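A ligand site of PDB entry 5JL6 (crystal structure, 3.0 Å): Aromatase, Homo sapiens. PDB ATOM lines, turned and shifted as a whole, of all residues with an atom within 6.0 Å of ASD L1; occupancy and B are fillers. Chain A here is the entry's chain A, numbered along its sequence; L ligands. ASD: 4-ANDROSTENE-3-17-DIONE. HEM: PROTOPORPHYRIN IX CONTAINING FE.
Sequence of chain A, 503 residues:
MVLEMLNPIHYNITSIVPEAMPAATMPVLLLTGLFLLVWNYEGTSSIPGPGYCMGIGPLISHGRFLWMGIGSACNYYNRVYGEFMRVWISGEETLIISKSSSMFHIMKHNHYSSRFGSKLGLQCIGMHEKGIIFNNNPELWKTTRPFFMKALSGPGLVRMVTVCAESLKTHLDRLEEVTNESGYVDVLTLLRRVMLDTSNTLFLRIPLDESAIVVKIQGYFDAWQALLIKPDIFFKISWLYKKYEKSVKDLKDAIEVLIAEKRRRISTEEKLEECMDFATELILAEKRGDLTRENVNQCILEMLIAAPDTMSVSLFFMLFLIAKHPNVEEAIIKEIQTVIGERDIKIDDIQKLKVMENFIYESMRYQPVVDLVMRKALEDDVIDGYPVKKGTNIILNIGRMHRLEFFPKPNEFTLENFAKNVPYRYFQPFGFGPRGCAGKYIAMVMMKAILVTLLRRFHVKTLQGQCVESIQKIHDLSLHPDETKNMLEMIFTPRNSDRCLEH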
ATOM      1  N   ARG A 115      -1.663  -3.214  23.313  1.00  0.00           N
ATOM      2  CA  ARG A 115      -2.473  -2.065  22.941  1.00  0.00           C
ATOM      3  C   ARG A 115      -3.683  -2.023  23.880  1.00  0.00           C
ATOM      4  O   ARG A 115      -3.645  -2.614  24.967  1.00  0.00           O
ATOM      5  CB  ARG A 115      -2.887  -2.169  21.464  1.00  0.00           C
ATOM      6  CG  ARG A 115      -1.745  -2.505  20.535  1.00  0.00           C
ATOM      7  CD  ARG A 115      -2.034  -2.089  19.096  1.00  0.00           C
ATOM      8  NE  ARG A 115      -0.952  -2.539  18.229  1.00  0.00           N
ATOM      9  CZ  ARG A 115       0.210  -1.903  18.030  1.00  0.00           C
ATOM     10  NH1 ARG A 115       0.469  -0.728  18.603  1.00  0.00           N
ATOM     11  NH2 ARG A 115       1.112  -2.450  17.227  1.00  0.00           N
ATOM     12  N   ILE A 133      -2.790  -7.503  15.576  1.00  0.00           N
ATOM     13  CA  ILE A 133      -2.790  -6.032  15.589  1.00  0.00           C
ATOM     14  C   ILE A 133      -3.318  -5.512  16.921  1.00  0.00           C
ATOM     15  O   ILE A 133      -2.636  -4.736  17.574  1.00  0.00           O
ATOM     16  CB  ILE A 133      -3.600  -5.396  14.439  1.00  0.00           C
ATOM     17  CG1 ILE A 133      -3.062  -5.832  13.064  1.00  0.00           C
ATOM     18  CG2 ILE A 133      -3.497  -3.874  14.507  1.00  0.00           C
ATOM     19  CD1 ILE A 133      -4.055  -5.613  11.951  1.00  0.00           C
ATOM     20  N   PHE A 134      -4.525  -5.953  17.308  1.00  0.00           N
ATOM     21  CA  PHE A 134      -5.097  -5.577  18.619  1.00  0.00           C
ATOM     22  C   PHE A 134      -5.270  -6.780  19.567  1.00  0.00           C
ATOM     23  O   PHE A 134      -6.137  -6.794  20.454  1.00  0.00           O
ATOM     24  CB  PHE A 134      -6.402  -4.775  18.429  1.00  0.00           C
ATOM     25  CG  PHE A 134      -6.174  -3.305  18.220  1.00  0.00           C
ATOM     26  CD1 PHE A 134      -6.048  -2.769  16.948  1.00  0.00           C
ATOM     27  CD2 PHE A 134      -6.066  -2.455  19.319  1.00  0.00           C
ATOM     28  CE1 PHE A 134      -5.809  -1.406  16.774  1.00  0.00           C
ATOM     29  CE2 PHE A 134      -5.836  -1.089  19.141  1.00  0.00           C
ATOM     30  CZ  PHE A 134      -5.702  -0.568  17.866  1.00  0.00           C
ATOM     31  N   PHE A 221     -12.797  -2.046   8.105  1.00  0.00           N
ATOM     32  CA  PHE A 221     -12.030  -0.990   8.725  1.00  0.00           C
ATOM     33  C   PHE A 221     -12.944   0.036   9.383  1.00  0.00           C
ATOM     34  O   PHE A 221     -12.685   0.453  10.515  1.00  0.00           O
ATOM     35  CB  PHE A 221     -11.091  -0.280   7.753  1.00  0.00           C
ATOM     36  CG  PHE A 221     -10.192   0.725   8.423  1.00  0.00           C
ATOM     37  CD1 PHE A 221      -8.960   0.336   8.937  1.00  0.00           C
ATOM     38  CD2 PHE A 221     -10.612   2.044   8.628  1.00  0.00           C
ATOM     39  CE1 PHE A 221      -8.147   1.243   9.609  1.00  0.00           C
ATOM     40  CE2 PHE A 221      -9.805   2.962   9.295  1.00  0.00           C
ATOM     41  CZ  PHE A 221      -8.564   2.563   9.781  1.00  0.00           C
ATOM     42  N   TRP A 224     -14.134  -1.453  12.678  1.00  0.00           N
ATOM     43  CA  TRP A 224     -12.979  -1.416  13.588  1.00  0.00           C
ATOM     44  C   TRP A 224     -12.777   0.006  14.121  1.00  0.00           C
ATOM     45  O   TRP A 224     -12.697   0.214  15.319  1.00  0.00           O
ATOM     46  CB  TRP A 224     -11.744  -1.956  12.828  1.00  0.00           C
ATOM     47  CG  TRP A 224     -10.401  -1.861  13.469  1.00  0.00           C
ATOM     48  CD1 TRP A 224     -10.092  -1.543  14.759  1.00  0.00           C
ATOM     49  CD2 TRP A 224      -9.164  -2.143  12.828  1.00  0.00           C
ATOM     50  NE1 TRP A 224      -8.734  -1.582  14.953  1.00  0.00           N
ATOM     51  CE2 TRP A 224      -8.140  -1.963  13.774  1.00  0.00           C
ATOM     52  CE3 TRP A 224      -8.816  -2.533  11.533  1.00  0.00           C
ATOM     53  CZ2 TRP A 224      -6.788  -2.143  13.464  1.00  0.00           C
ATOM     54  CZ3 TRP A 224      -7.477  -2.720  11.221  1.00  0.00           C
ATOM     55  CH2 TRP A 224      -6.475  -2.514  12.184  1.00  0.00           C
ATOM     56  N   GLU A 302      -6.227 -10.502   8.918  1.00  0.00           N
ATOM     57  CA  GLU A 302      -5.386  -9.350   9.274  1.00  0.00           C
ATOM     58  C   GLU A 302      -4.244  -9.089   8.279  1.00  0.00           C
ATOM     59  O   GLU A 302      -3.903  -7.932   8.041  1.00  0.00           O
ATOM     60  CB  GLU A 302      -4.870  -9.444  10.718  1.00  0.00           C
ATOM     61  CG  GLU A 302      -5.945  -9.072  11.753  1.00  0.00           C
ATOM     62  CD  GLU A 302      -5.454  -9.022  13.197  1.00  0.00           C
ATOM     63  OE1 GLU A 302      -4.228  -9.170  13.442  1.00  0.00           O
ATOM     64  OE2 GLU A 302      -6.302  -8.829  14.129  1.00  0.00           O
ATOM     65  N   ILE A 305      -5.991  -7.416   4.921  1.00  0.00           N
ATOM     66  CA  ILE A 305      -6.456  -6.042   5.057  1.00  0.00           C
ATOM     67  C   ILE A 305      -5.328  -5.039   5.190  1.00  0.00           C
ATOM     68  O   ILE A 305      -5.511  -3.877   4.836  1.00  0.00           O
ATOM     69  CB  ILE A 305      -7.445  -5.854   6.239  1.00  0.00           C
ATOM     70  CG1 ILE A 305      -6.785  -6.077   7.600  1.00  0.00           C
ATOM     71  CG2 ILE A 305      -8.640  -6.781   6.076  1.00  0.00           C
ATOM     72  CD1 ILE A 305      -7.658  -5.674   8.763  1.00  0.00           C
ATOM     73  N   ALA A 306      -4.172  -5.478   5.690  1.00  0.00           N
ATOM     74  CA  ALA A 306      -3.127  -4.568   6.163  1.00  0.00           C
ATOM     75  C   ALA A 306      -2.702  -3.549   5.132  1.00  0.00           C
ATOM     76  O   ALA A 306      -2.705  -2.344   5.388  1.00  0.00           O
ATOM     77  CB  ALA A 306      -1.910  -5.348   6.654  1.00  0.00           C
ATOM     78  N   ALA A 307      -2.331  -4.059   3.961  1.00  0.00           N
ATOM     79  CA  ALA A 307      -1.828  -3.192   2.903  1.00  0.00           C
ATOM     80  C   ALA A 307      -2.939  -2.303   2.321  1.00  0.00           C
ATOM     81  O   ALA A 307      -2.784  -1.083   2.271  1.00  0.00           O
ATOM     82  CB  ALA A 307      -1.092  -4.005   1.833  1.00  0.00           C
ATOM     83  N   ASP A 309      -5.528  -1.136   3.702  1.00  0.00           N
ATOM     84  CA  ASP A 309      -5.916  -0.090   4.648  1.00  0.00           C
ATOM     85  C   ASP A 309      -4.929   1.059   4.656  1.00  0.00           C
ATOM     86  O   ASP A 309      -5.329   2.216   4.675  1.00  0.00           O
ATOM     87  CB  ASP A 309      -6.053  -0.649   6.061  1.00  0.00           C
ATOM     88  CG  ASP A 309      -7.225  -1.619   6.215  1.00  0.00           C
ATOM     89  OD1 ASP A 309      -8.187  -1.556   5.423  1.00  0.00           O
ATOM     90  OD2 ASP A 309      -7.175  -2.440   7.141  1.00  0.00           O
ATOM     91  N   THR A 310      -3.644   0.738   4.618  1.00  0.00           N
ATOM     92  CA  THR A 310      -2.604   1.701   4.955  1.00  0.00           C
ATOM     93  C   THR A 310      -1.699   2.136   3.794  1.00  0.00           C
ATOM     94  O   THR A 310      -1.375   3.315   3.689  1.00  0.00           O
ATOM     95  CB  THR A 310      -1.741   1.136   6.081  1.00  0.00           C
ATOM     96  OG1 THR A 310      -1.190  -0.135   5.682  1.00  0.00           O
ATOM     97  CG2 THR A 310      -2.592   0.959   7.321  1.00  0.00           C
ATOM     98  N   VAL A 370      -0.757   6.805   9.531  1.00  0.00           N
ATOM     99  CA  VAL A 370      -0.719   6.230  10.869  1.00  0.00           C
ATOM    100  C   VAL A 370       0.003   7.245  11.751  1.00  0.00           C
ATOM    101  O   VAL A 370       1.196   7.140  12.023  1.00  0.00           O
ATOM    102  CB  VAL A 370      -0.037   4.852  10.881  1.00  0.00           C
ATOM    103  CG1 VAL A 370      -0.247   4.168  12.222  1.00  0.00           C
ATOM    104  CG2 VAL A 370      -0.576   3.981   9.749  1.00  0.00           C
ATOM    105  N   LEU A 372      -0.769   7.991  14.894  1.00  0.00           N
ATOM    106  CA  LEU A 372      -0.740   7.654  16.311  1.00  0.00           C
ATOM    107  C   LEU A 372      -0.804   6.164  16.568  1.00  0.00           C
ATOM    108  O   LEU A 372      -1.312   5.406  15.759  1.00  0.00           O
ATOM    109  CB  LEU A 372      -1.870   8.386  17.036  1.00  0.00           C
ATOM    110  CG  LEU A 372      -3.287   8.075  16.551  1.00  0.00           C
ATOM    111  CD1 LEU A 372      -3.953   6.940  17.332  1.00  0.00           C
ATOM    112  CD2 LEU A 372      -4.110   9.341  16.689  1.00  0.00           C
ATOM    113  N   VAL A 373      -0.270   5.791  17.727  1.00  0.00           N
ATOM    114  CA  VAL A 373      -0.017   4.405  18.106  1.00  0.00           C
ATOM    115  C   VAL A 373      -0.563   4.189  19.500  1.00  0.00           C
ATOM    116  O   VAL A 373      -0.267   4.973  20.403  1.00  0.00           O
ATOM    117  CB  VAL A 373       1.493   4.111  18.137  1.00  0.00           C
ATOM    118  CG1 VAL A 373       1.756   2.689  18.600  1.00  0.00           C
ATOM    119  CG2 VAL A 373       2.110   4.385  16.774  1.00  0.00           C
ATOM    120  N   MET A 374      -1.300   3.104  19.688  1.00  0.00           N
ATOM    121  CA  MET A 374      -1.948   2.817  20.957  1.00  0.00           C
ATOM    122  C   MET A 374      -1.158   1.714  21.618  1.00  0.00           C
ATOM    123  O   MET A 374      -0.938   0.667  21.015  1.00  0.00           O
ATOM    124  CB  MET A 374      -3.396   2.397  20.710  1.00  0.00           C
ATOM    125  CG  MET A 374      -4.218   3.486  20.033  1.00  0.00           C
ATOM    126  SD  MET A 374      -5.886   2.966  19.625  1.00  0.00           S
ATOM    127  CE  MET A 374      -6.641   3.012  21.241  1.00  0.00           C
ATOM    128  N   ARG A 375      -0.705   1.978  22.850  1.00  0.00           N
ATOM    129  CA  ARG A 375       0.007   0.985  23.667  1.00  0.00           C
ATOM    130  C   ARG A 375      -0.574   0.900  25.076  1.00  0.00           C
ATOM    131  O   ARG A 375      -1.490   1.640  25.435  1.00  0.00           O
ATOM    132  CB  ARG A 375       1.493   1.317  23.737  1.00  0.00           C
ATOM    133  CG  ARG A 375       2.191   1.348  22.387  1.00  0.00           C
ATOM    134  CD  ARG A 375       2.126   0.028  21.629  1.00  0.00           C
ATOM    135  NE  ARG A 375       3.265  -0.151  20.736  1.00  0.00           N
ATOM    136  CZ  ARG A 375       4.488  -0.528  21.119  1.00  0.00           C
ATOM    137  NH1 ARG A 375       4.752  -0.753  22.405  1.00  0.00           N
ATOM    138  NH2 ARG A 375       5.448  -0.680  20.216  1.00  0.00           N
ATOM    139  N   LEU A 477      -9.019   6.942  13.762  1.00  0.00           N
ATOM    140  CA  LEU A 477      -8.029   5.891  14.070  1.00  0.00           C
ATOM    141  C   LEU A 477      -6.772   6.142  13.249  1.00  0.00           C
ATOM    142  O   LEU A 477      -5.660   6.226  13.790  1.00  0.00           O
ATOM    143  CB  LEU A 477      -8.566   4.476  13.746  1.00  0.00           C
ATOM    144  CG  LEU A 477      -8.358   3.301  14.720  1.00  0.00           C
ATOM    145  CD1 LEU A 477      -8.204   2.007  13.941  1.00  0.00           C
ATOM    146  CD2 LEU A 477      -7.216   3.490  15.711  1.00  0.00           C
ATOM    147  N   SER A 478      -6.961   6.239  11.938  1.00  0.00           N
ATOM    148  CA  SER A 478      -5.926   6.668  11.021  1.00  0.00           C
ATOM    149  C   SER A 478      -6.272   8.071  10.529  1.00  0.00           C
ATOM    150  O   SER A 478      -7.281   8.654  10.947  1.00  0.00           O
ATOM    151  CB  SER A 478      -5.806   5.679   9.846  1.00  0.00           C
ATOM    152  OG  SER A 478      -6.983   5.662   9.056  1.00  0.00           O
HETATM  153  C1  ASD L   1      -2.336  -2.063  11.082  1.00  0.00           C
HETATM  154  C10 ASD L   1      -2.514  -0.536  11.230  1.00  0.00           C
HETATM  155  C11 ASD L   1      -1.636  -0.755  13.668  1.00  0.00           C
HETATM  156  C12 ASD L   1      -1.787  -0.344  15.126  1.00  0.00           C
HETATM  157  C13 ASD L   1      -2.025   1.152  15.236  1.00  0.00           C
HETATM  158  C14 ASD L   1      -3.286   1.445  14.460  1.00  0.00           C
HETATM  159  C15 ASD L   1      -3.751   2.810  14.959  1.00  0.00           C
HETATM  160  C16 ASD L   1      -3.433   2.801  16.453  1.00  0.00           C
HETATM  161  C17 ASD L   1      -2.431   1.681  16.579  1.00  0.00           C
HETATM  162  C18 ASD L   1      -0.798   1.970  14.824  1.00  0.00           C
HETATM  163  C19 ASD L   1      -1.274   0.143  10.666  1.00  0.00           C
HETATM  164  C2  ASD L   1      -2.681  -2.643   9.721  1.00  0.00           C
HETATM  165  C3  ASD L   1      -3.997  -2.124   9.229  1.00  0.00           C
HETATM  166  C4  ASD L   1      -4.451  -0.774   9.613  1.00  0.00           C
HETATM  167  C5  ASD L   1      -3.752  -0.028  10.497  1.00  0.00           C
HETATM  168  C6  ASD L   1      -4.229   1.376  10.762  1.00  0.00           C
HETATM  169  C7  ASD L   1      -4.393   1.599  12.250  1.00  0.00           C
HETATM  170  C8  ASD L   1      -3.109   1.241  12.980  1.00  0.00           C
HETATM  171  C9  ASD L   1      -2.750  -0.234  12.731  1.00  0.00           C
HETATM  172  O1  ASD L   1      -4.710  -2.831   8.538  1.00  0.00           O
HETATM  173  O2  ASD L   1      -2.019   1.267  17.651  1.00  0.00           O
HETATM  174  CHA HEM L   2       1.601  -2.101  13.232  1.00  0.00           C
HETATM  175  CHB HEM L   2       2.605   1.660  10.406  1.00  0.00           C
HETATM  176  CHC HEM L   2       2.147  -1.154   6.503  1.00  0.00           C
HETATM  177  CHD HEM L   2       1.386  -4.939   9.323  1.00  0.00           C
HETATM  178  C1A HEM L   2       1.941  -0.856  12.790  1.00  0.00           C
HETATM  179  C2A HEM L   2       2.210   0.246  13.632  1.00  0.00           C
HETATM  180  C3A HEM L   2       2.499   1.299  12.837  1.00  0.00           C
HETATM  181  C4A HEM L   2       2.422   0.860  11.500  1.00  0.00           C
HETATM  182  CMA HEM L   2       2.847   2.689  13.349  1.00  0.00           C
HETATM  183  CAA HEM L   2       2.201   0.267  15.149  1.00  0.00           C
HETATM  184  CBA HEM L   2       3.564  -0.264  15.626  1.00  0.00           C
HETATM  185  CGA HEM L   2       3.797   0.044  17.088  1.00  0.00           C
HETATM  186  O1A HEM L   2       2.885  -0.077  17.927  1.00  0.00           O
HETATM  187  O2A HEM L   2       4.921   0.404  17.474  1.00  0.00           O
HETATM  188  C1B HEM L   2       2.526   1.225   9.078  1.00  0.00           C
HETATM  189  C2B HEM L   2       2.692   2.079   7.956  1.00  0.00           C
HETATM  190  C3B HEM L   2       2.572   1.306   6.834  1.00  0.00           C
HETATM  191  C4B HEM L   2       2.312  -0.066   7.341  1.00  0.00           C
HETATM  192  CMB HEM L   2       2.973   3.557   8.052  1.00  0.00           C
HETATM  193  CAB HEM L   2       2.669   1.635   5.379  1.00  0.00           C
HETATM  194  CBB HEM L   2       2.905   2.820   4.851  1.00  0.00           C
HETATM  195  C1C HEM L   2       1.941  -2.454   6.908  1.00  0.00           C
HETATM  196  C2C HEM L   2       1.837  -3.581   6.059  1.00  0.00           C
HETATM  197  C3C HEM L   2       1.622  -4.692   6.878  1.00  0.00           C
HETATM  198  C4C HEM L   2       1.595  -4.189   8.213  1.00  0.00           C
HETATM  199  CMC HEM L   2       1.977  -3.551   4.561  1.00  0.00           C
HETATM  200  CAC HEM L   2       1.431  -6.138   6.516  1.00  0.00           C
HETATM  201  CBC HEM L   2       1.407  -6.638   5.276  1.00  0.00           C
HETATM  202  C1D HEM L   2       1.366  -4.409  10.605  1.00  0.00           C
HETATM  203  C2D HEM L   2       1.075  -5.272  11.748  1.00  0.00           C
HETATM  204  C3D HEM L   2       1.134  -4.514  12.847  1.00  0.00           C
HETATM  205  C4D HEM L   2       1.453  -3.153  12.350  1.00  0.00           C
HETATM  206  CMD HEM L   2       0.779  -6.749  11.715  1.00  0.00           C
HETATM  207  CAD HEM L   2       0.874  -4.954  14.263  1.00  0.00           C
HETATM  208  CBD HEM L   2       2.132  -5.362  15.018  1.00  0.00           C
HETATM  209  CGD HEM L   2       1.766  -5.796  16.422  1.00  0.00           C
HETATM  210  O1D HEM L   2       2.400  -6.722  16.964  1.00  0.00           O
HETATM  211  O2D HEM L   2       0.847  -5.226  17.042  1.00  0.00           O
HETATM  212  NA  HEM L   2       2.095  -0.464  11.484  1.00  0.00           N
HETATM  213  NB  HEM L   2       2.325  -0.019   8.663  1.00  0.00           N
HETATM  214  NC  HEM L   2       1.796  -2.845   8.193  1.00  0.00           N
HETATM  215  ND  HEM L   2       1.602  -3.138  11.008  1.00  0.00           N
HETATM  216 FE   HEM L   2       1.963  -1.645   9.896  1.00  0.00          FE
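An oxygen (O1) of ASD L1 lies close to the side-chain carboxylate (OD2) of Asp 309, at 2.9 Å. Merely in contact with ASD L1: Ile 133 (3.7 Å), Trp 224 (3.7 Å), Ile 305 (3.9 Å), Ala 306 (3.3 Å), Thr 310 (3.4 Å), Val 370 (3.5 Å), Leu 372 (3.4 Å), Val 373 (3.7 Å) and Leu 477 (3.6 Å). 12 residues have an atom within 4 Å of ASD L1: Arg 115, Ile 133, Trp 224, Ile 305, Ala 306, Asp 309, Thr 310, Val 370, Leu 372, Val 373, Met 374 and Leu 477.
The backbone carbonyl oxygen (O) of Ile 133 lies within hydrogen-bond range of the guanidinium group (NE) of Arg 115 (2.8 Å). The side-chain carboxylate (OE1) of Glu 302 lies within hydrogen-bond range of the backbone NH (N) of Ile 133 (3.1 Å). The guanidinium group (NH1) of Arg 115 lies within hydrogen-bond range of the backbone carbonyl oxygen (O) of Met 374 (3.1 Å). The backbone carbonyl oxygen of Ala 306 lies within hydrogen-bond range of the side-chain hydroxyl of Thr 310, 2.7 Å away.
The guanidinium group of Arg 115 lies within salt-bridge range of an oxygen (O1A) of HEM L2. The backbone NH (N) of Met 374 is in hydrogen-bond range of an oxygen (O2) of ASD L1 (2.8 Å). An oxygen (O1A) of HEM L2 lies within salt-bridge range of the guanidinium group (NE) of Arg 375 (2.8 Å). O2 of ASD L1 sits at hydrogen-bond distance from NH1 of Arg 115, at 3.3 Å.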
